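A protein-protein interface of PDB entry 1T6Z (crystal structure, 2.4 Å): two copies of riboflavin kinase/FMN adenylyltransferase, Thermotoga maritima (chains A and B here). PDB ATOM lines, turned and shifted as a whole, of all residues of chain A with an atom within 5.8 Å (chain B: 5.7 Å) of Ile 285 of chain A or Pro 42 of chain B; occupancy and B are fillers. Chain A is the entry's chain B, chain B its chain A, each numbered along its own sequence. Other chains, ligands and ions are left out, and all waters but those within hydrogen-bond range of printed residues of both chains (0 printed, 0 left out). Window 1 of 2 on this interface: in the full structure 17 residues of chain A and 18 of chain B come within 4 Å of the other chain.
No position is printed for both chains.
Of the printed residues of chain B, Ile 285 of chain A touches Pro 42 (3.4 Å) and Phe 74 (3.98 Å). Printed residues of chain B within 4 Å of Phe 289 of chain A: Phe 45 and Lys 78. Of chain A, only Ile 285 (3.4 Å) comes within 4 Å of Pro 42 of chain B. Of the printed residues of chain A, Phe 45 of chain B touches Lys 288 (3.7 Å) and Phe 289 (3.9 Å). The nearest printed residue of chain B that does not touch Ile 285 of chain A is Leu 46 of chain B (4.3 Å). The nearest printed residue of chain A that does not touch Pro 42 of chain B is Ile 281 of chain A (6.6 Å). The nearest printed residue of chain B that does not touch Lys 288 of chain A is Tyr 44 of chain B (7.4 Å).
Hydrophobic or aromatic side chains of chain A that line the printed part of chain B: Ile 284, Ile 285 and Phe 289. Of the 9 printed residues of chain B, 5 touch a printed residue of chain A. Among the printed residues, 8 pairs touch across the chains. Among the printed residues, no Asp or Glu carboxylate lies within 4 Å of a Lys or Arg side-chain nitrogen of the other chain.
The backbone carbonyl oxygen (O) of Ile 284 of chain A is in hydrogen-bond range of the side-chain hydroxyl (OG) of Ser 287 of chain A (2.5 Å). The side-chain amide nitrogen (ND2) of Asn 286 of chain A lies within hydrogen-bond range of the side-chain carboxylate (OD2) of Asp 282 of chain A, at 2.7 Å.
Leu 46 of chain B touches Ile 284 of chain A. Ile 285 of chain A touches Pro 42 of chain B. Ile 285 of chain A touches Phe 74 of chain B. Asn 286 of chain A touches Lys 78 of chain B. CG of Lys 288 of chain A touches O of Phe 45 of chain B, 3.7 Å away. Lys 288 of chain A touches Leu 46 of chain B. CD1 of Phe 45 of chain B touches CE2 of Phe 289 of chain A, at 3.9 Å. Phe 289 of chain A touches Lys 78 of chain B.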
ATOM      1  N   MET A 280     -16.185  -5.633 -19.326  1.00  0.00           N
ATOM      2  CA  MET A 280     -16.618  -6.733 -20.180  1.00  0.00           C
ATOM      3  C   MET A 280     -17.477  -7.707 -19.382  1.00  0.00           C
ATOM      4  O   MET A 280     -18.461  -8.260 -19.902  1.00  0.00           O
ATOM      5  CB  MET A 280     -15.408  -7.454 -20.763  1.00  0.00           C
ATOM      6  CG  MET A 280     -14.563  -6.589 -21.663  1.00  0.00           C
ATOM      7  SD  MET A 280     -13.045  -7.414 -22.142  1.00  0.00           S
ATOM      8  CE  MET A 280     -13.604  -8.182 -23.647  1.00  0.00           C
ATOM      9  N   ILE A 281     -17.105  -7.910 -18.115  1.00  0.00           N
ATOM     10  CA  ILE A 281     -17.857  -8.799 -17.241  1.00  0.00           C
ATOM     11  C   ILE A 281     -19.259  -8.234 -17.081  1.00  0.00           C
ATOM     12  O   ILE A 281     -20.234  -8.975 -17.101  1.00  0.00           O
ATOM     13  CB  ILE A 281     -17.195  -8.955 -15.854  1.00  0.00           C
ATOM     14  CG1 ILE A 281     -15.852  -9.669 -15.994  1.00  0.00           C
ATOM     15  CG2 ILE A 281     -18.098  -9.768 -14.942  1.00  0.00           C
ATOM     16  CD1 ILE A 281     -15.074  -9.794 -14.712  1.00  0.00           C
ATOM     17  N   ASP A 282     -19.363  -6.914 -16.944  1.00  0.00           N
ATOM     18  CA  ASP A 282     -20.671  -6.282 -16.818  1.00  0.00           C
ATOM     19  C   ASP A 282     -21.422  -6.439 -18.150  1.00  0.00           C
ATOM     20  O   ASP A 282     -22.601  -6.810 -18.172  1.00  0.00           O
ATOM     21  CB  ASP A 282     -20.514  -4.798 -16.469  1.00  0.00           C
ATOM     22  CG  ASP A 282     -21.797  -4.183 -15.920  1.00  0.00           C
ATOM     23  OD1 ASP A 282     -22.135  -4.449 -14.741  1.00  0.00           O
ATOM     24  OD2 ASP A 282     -22.467  -3.446 -16.677  1.00  0.00           O
ATOM     25  N   ASP A 283     -20.728  -6.164 -19.257  1.00  0.00           N
ATOM     26  CA  ASP A 283     -21.322  -6.284 -20.594  1.00  0.00           C
ATOM     27  C   ASP A 283     -21.963  -7.658 -20.795  1.00  0.00           C
ATOM     28  O   ASP A 283     -23.110  -7.767 -21.240  1.00  0.00           O
ATOM     29  CB  ASP A 283     -20.264  -6.046 -21.684  1.00  0.00           C
ATOM     30  CG  ASP A 283     -19.934  -4.559 -21.881  1.00  0.00           C
ATOM     31  OD1 ASP A 283     -20.827  -3.711 -21.643  1.00  0.00           O
ATOM     32  OD2 ASP A 283     -18.792  -4.243 -22.295  1.00  0.00           O
ATOM     33  N   ILE A 284     -21.216  -8.700 -20.449  1.00  0.00           N
ATOM     34  CA  ILE A 284     -21.710 -10.062 -20.586  1.00  0.00           C
ATOM     35  C   ILE A 284     -23.023 -10.282 -19.837  1.00  0.00           C
ATOM     36  O   ILE A 284     -23.963 -10.877 -20.362  1.00  0.00           O
ATOM     37  CB  ILE A 284     -20.677 -11.083 -20.059  1.00  0.00           C
ATOM     38  CG1 ILE A 284     -19.410 -11.021 -20.906  1.00  0.00           C
ATOM     39  CG2 ILE A 284     -21.275 -12.476 -20.059  1.00  0.00           C
ATOM     40  CD1 ILE A 284     -18.325 -12.002 -20.486  1.00  0.00           C
ATOM     41  N   ILE A 285     -23.073  -9.807 -18.600  1.00  0.00           N
ATOM     42  CA  ILE A 285     -24.254  -9.969 -17.770  1.00  0.00           C
ATOM     43  C   ILE A 285     -25.448  -9.182 -18.278  1.00  0.00           C
ATOM     44  O   ILE A 285     -26.573  -9.677 -18.263  1.00  0.00           O
ATOM     45  CB  ILE A 285     -23.975  -9.536 -16.321  1.00  0.00           C
ATOM     46  CG1 ILE A 285     -22.932 -10.461 -15.689  1.00  0.00           C
ATOM     47  CG2 ILE A 285     -25.271  -9.548 -15.518  1.00  0.00           C
ATOM     48  CD1 ILE A 285     -22.575 -10.086 -14.263  1.00  0.00           C
ATOM     49  N   ASN A 286     -25.225  -7.955 -18.725  1.00  0.00           N
ATOM     50  CA  ASN A 286     -26.347  -7.164 -19.199  1.00  0.00           C
ATOM     51  C   ASN A 286     -26.815  -7.544 -20.591  1.00  0.00           C
ATOM     52  O   ASN A 286     -27.927  -7.200 -20.991  1.00  0.00           O
ATOM     53  CB  ASN A 286     -26.015  -5.677 -19.130  1.00  0.00           C
ATOM     54  CG  ASN A 286     -25.919  -5.180 -17.703  1.00  0.00           C
ATOM     55  OD1 ASN A 286     -26.791  -5.462 -16.881  1.00  0.00           O
ATOM     56  ND2 ASN A 286     -24.863  -4.437 -17.400  1.00  0.00           N
ATOM     57  N   SER A 287     -25.976  -8.270 -21.322  1.00  0.00           N
ATOM     58  CA  SER A 287     -26.334  -8.692 -22.666  1.00  0.00           C
ATOM     59  C   SER A 287     -27.516  -9.666 -22.639  1.00  0.00           C
ATOM     60  O   SER A 287     -28.273  -9.758 -23.603  1.00  0.00           O
ATOM     61  CB  SER A 287     -25.133  -9.351 -23.347  1.00  0.00           C
ATOM     62  OG  SER A 287     -24.789 -10.571 -22.716  1.00  0.00           O
ATOM     63  N   LYS A 288     -27.680 -10.380 -21.530  1.00  0.00           N
ATOM     64  CA  LYS A 288     -28.769 -11.347 -21.393  1.00  0.00           C
ATOM     65  C   LYS A 288     -30.161 -10.707 -21.415  1.00  0.00           C
ATOM     66  O   LYS A 288     -31.169 -11.394 -21.217  1.00  0.00           O
ATOM     67  CB  LYS A 288     -28.593 -12.174 -20.105  1.00  0.00           C
ATOM     68  CG  LYS A 288     -27.558 -13.300 -20.196  1.00  0.00           C
ATOM     69  CD  LYS A 288     -26.181 -12.769 -20.557  1.00  0.00           C
ATOM     70  CE  LYS A 288     -25.121 -13.870 -20.615  1.00  0.00           C
ATOM     71  NZ  LYS A 288     -25.346 -14.891 -21.682  1.00  0.00           N
ATOM     72  N   PHE A 289     -30.208  -9.397 -21.655  1.00  0.00           N
ATOM     73  CA  PHE A 289     -31.467  -8.651 -21.725  1.00  0.00           C
ATOM     74  C   PHE A 289     -31.266  -7.189 -22.107  1.00  0.00           C
ATOM     75  O   PHE A 289     -30.162  -6.650 -22.005  1.00  0.00           O
ATOM     76  CB  PHE A 289     -32.237  -8.731 -20.396  1.00  0.00           C
ATOM     77  CG  PHE A 289     -31.370  -8.625 -19.166  1.00  0.00           C
ATOM     78  CD1 PHE A 289     -30.557  -7.517 -18.954  1.00  0.00           C
ATOM     79  CD2 PHE A 289     -31.374  -9.643 -18.214  1.00  0.00           C
ATOM     80  CE1 PHE A 289     -29.758  -7.425 -17.810  1.00  0.00           C
ATOM     81  CE2 PHE A 289     -30.581  -9.562 -17.071  1.00  0.00           C
ATOM     82  CZ  PHE A 289     -29.771  -8.451 -16.868  1.00  0.00           C
ATOM     83  N   TYR B  40     -30.747 -11.469  -6.758  1.00  0.00           N
ATOM     84  CA  TYR B  40     -29.977 -12.447  -7.507  1.00  0.00           C
ATOM     85  C   TYR B  40     -28.527 -12.019  -7.615  1.00  0.00           C
ATOM     86  O   TYR B  40     -28.232 -10.824  -7.718  1.00  0.00           O
ATOM     87  CB  TYR B  40     -30.499 -12.591  -8.949  1.00  0.00           C
ATOM     88  CG  TYR B  40     -31.956 -12.908  -9.068  1.00  0.00           C
ATOM     89  CD1 TYR B  40     -32.468 -14.104  -8.589  1.00  0.00           C
ATOM     90  CD2 TYR B  40     -32.834 -11.987  -9.613  1.00  0.00           C
ATOM     91  CE1 TYR B  40     -33.825 -14.367  -8.641  1.00  0.00           C
ATOM     92  CE2 TYR B  40     -34.197 -12.241  -9.669  1.00  0.00           C
ATOM     93  CZ  TYR B  40     -34.687 -13.427  -9.180  1.00  0.00           C
ATOM     94  OH  TYR B  40     -36.041 -13.650  -9.204  1.00  0.00           O
ATOM     95  N   PRO B  41     -27.602 -12.996  -7.596  1.00  0.00           N
ATOM     96  CA  PRO B  41     -26.180 -12.682  -7.713  1.00  0.00           C
ATOM     97  C   PRO B  41     -25.978 -12.480  -9.201  1.00  0.00           C
ATOM     98  O   PRO B  41     -26.836 -12.857 -10.002  1.00  0.00           O
ATOM     99  CB  PRO B  41     -25.503 -13.941  -7.184  1.00  0.00           C
ATOM    100  CG  PRO B  41     -26.464 -15.021  -7.596  1.00  0.00           C
ATOM    101  CD  PRO B  41     -27.801 -14.415  -7.235  1.00  0.00           C
ATOM    102  N   PRO B  42     -24.853 -11.885  -9.599  1.00  0.00           N
ATOM    103  CA  PRO B  42     -24.576 -11.641 -11.022  1.00  0.00           C
ATOM    104  C   PRO B  42     -24.552 -12.928 -11.851  1.00  0.00           C
ATOM    105  O   PRO B  42     -25.033 -12.963 -12.976  1.00  0.00           O
ATOM    106  CB  PRO B  42     -23.206 -10.953 -11.003  1.00  0.00           C
ATOM    107  CG  PRO B  42     -23.092 -10.417  -9.584  1.00  0.00           C
ATOM    108  CD  PRO B  42     -23.717 -11.493  -8.756  1.00  0.00           C
ATOM    109  N   GLU B  43     -23.989 -13.981 -11.272  1.00  0.00           N
ATOM    110  CA  GLU B  43     -23.863 -15.274 -11.935  1.00  0.00           C
ATOM    111  C   GLU B  43     -25.200 -15.926 -12.249  1.00  0.00           C
ATOM    112  O   GLU B  43     -25.282 -16.793 -13.100  1.00  0.00           O
ATOM    113  CB  GLU B  43     -23.032 -16.230 -11.067  1.00  0.00           C
ATOM    114  CG  GLU B  43     -21.580 -15.808 -10.808  1.00  0.00           C
ATOM    115  CD  GLU B  43     -21.429 -14.683  -9.776  1.00  0.00           C
ATOM    116  OE1 GLU B  43     -21.986 -14.804  -8.661  1.00  0.00           O
ATOM    117  OE2 GLU B  43     -20.733 -13.685 -10.081  1.00  0.00           O
ATOM    118  N   TYR B  44     -26.245 -15.521 -11.547  1.00  0.00           N
ATOM    119  CA  TYR B  44     -27.567 -16.087 -11.761  1.00  0.00           C
ATOM    120  C   TYR B  44     -27.985 -15.952 -13.212  1.00  0.00           C
ATOM    121  O   TYR B  44     -28.837 -16.684 -13.693  1.00  0.00           O
ATOM    122  CB  TYR B  44     -28.595 -15.356 -10.898  1.00  0.00           C
ATOM    123  CG  TYR B  44     -30.032 -15.803 -11.092  1.00  0.00           C
ATOM    124  CD1 TYR B  44     -30.552 -16.844 -10.360  1.00  0.00           C
ATOM    125  CD2 TYR B  44     -30.897 -15.113 -11.948  1.00  0.00           C
ATOM    126  CE1 TYR B  44     -31.904 -17.192 -10.440  1.00  0.00           C
ATOM    127  CE2 TYR B  44     -32.256 -15.458 -12.045  1.00  0.00           C
ATOM    128  CZ  TYR B  44     -32.742 -16.491 -11.276  1.00  0.00           C
ATOM    129  OH  TYR B  44     -34.081 -16.793 -11.274  1.00  0.00           O
ATOM    130  N   PHE B  45     -27.392 -15.013 -13.920  1.00  0.00           N
ATOM    131  CA  PHE B  45     -27.793 -14.824 -15.287  1.00  0.00           C
ATOM    132  C   PHE B  45     -26.959 -15.560 -16.322  1.00  0.00           C
ATOM    133  O   PHE B  45     -27.422 -15.814 -17.436  1.00  0.00           O
ATOM    134  CB  PHE B  45     -27.861 -13.325 -15.551  1.00  0.00           C
ATOM    135  CG  PHE B  45     -28.923 -12.649 -14.743  1.00  0.00           C
ATOM    136  CD1 PHE B  45     -30.268 -12.867 -15.032  1.00  0.00           C
ATOM    137  CD2 PHE B  45     -28.588 -11.849 -13.658  1.00  0.00           C
ATOM    138  CE1 PHE B  45     -31.272 -12.301 -14.257  1.00  0.00           C
ATOM    139  CE2 PHE B  45     -29.581 -11.277 -12.872  1.00  0.00           C
ATOM    140  CZ  PHE B  45     -30.930 -11.504 -13.172  1.00  0.00           C
ATOM    141  N   LEU B  46     -25.737 -15.915 -15.954  1.00  0.00           N
ATOM    142  CA  LEU B  46     -24.866 -16.642 -16.857  1.00  0.00           C
ATOM    143  C   LEU B  46     -25.442 -18.052 -17.052  1.00  0.00           C
ATOM    144  O   LEU B  46     -26.016 -18.628 -16.120  1.00  0.00           O
ATOM    145  CB  LEU B  46     -23.454 -16.673 -16.272  1.00  0.00           C
ATOM    146  CG  LEU B  46     -22.950 -15.250 -16.000  1.00  0.00           C
ATOM    147  CD1 LEU B  46     -21.481 -15.254 -15.576  1.00  0.00           C
ATOM    148  CD2 LEU B  46     -23.153 -14.415 -17.271  1.00  0.00           C
ATOM    149  N   PHE B  74     -32.002  -6.775  -8.102  1.00  0.00           N
ATOM    150  CA  PHE B  74     -30.857  -6.802  -8.990  1.00  0.00           C
ATOM    151  C   PHE B  74     -31.063  -5.903 -10.208  1.00  0.00           C
ATOM    152  O   PHE B  74     -30.157  -5.186 -10.639  1.00  0.00           O
ATOM    153  CB  PHE B  74     -30.614  -8.229  -9.479  1.00  0.00           C
ATOM    154  CG  PHE B  74     -29.606  -8.309 -10.573  1.00  0.00           C
ATOM    155  CD1 PHE B  74     -28.246  -8.370 -10.278  1.00  0.00           C
ATOM    156  CD2 PHE B  74     -30.010  -8.249 -11.901  1.00  0.00           C
ATOM    157  CE1 PHE B  74     -27.293  -8.363 -11.295  1.00  0.00           C
ATOM    158  CE2 PHE B  74     -29.075  -8.240 -12.925  1.00  0.00           C
ATOM    159  CZ  PHE B  74     -27.705  -8.298 -12.623  1.00  0.00           C
ATOM    160  N   LYS B  78     -28.190  -3.019 -10.546  1.00  0.00           N
ATOM    161  CA  LYS B  78     -27.024  -3.378 -11.341  1.00  0.00           C
ATOM    162  C   LYS B  78     -26.404  -2.203 -12.082  1.00  0.00           C
ATOM    163  O   LYS B  78     -25.185  -2.152 -12.251  1.00  0.00           O
ATOM    164  CB  LYS B  78     -27.355  -4.506 -12.326  1.00  0.00           C
ATOM    165  CG  LYS B  78     -28.448  -4.174 -13.332  1.00  0.00           C
ATOM    166  CD  LYS B  78     -28.526  -5.220 -14.430  1.00  0.00           C
ATOM    167  CE  LYS B  78     -29.795  -5.088 -15.228  1.00  0.00           C
ATOM    168  NZ  LYS B  78     -29.914  -3.704 -15.751  1.00  0.00           N
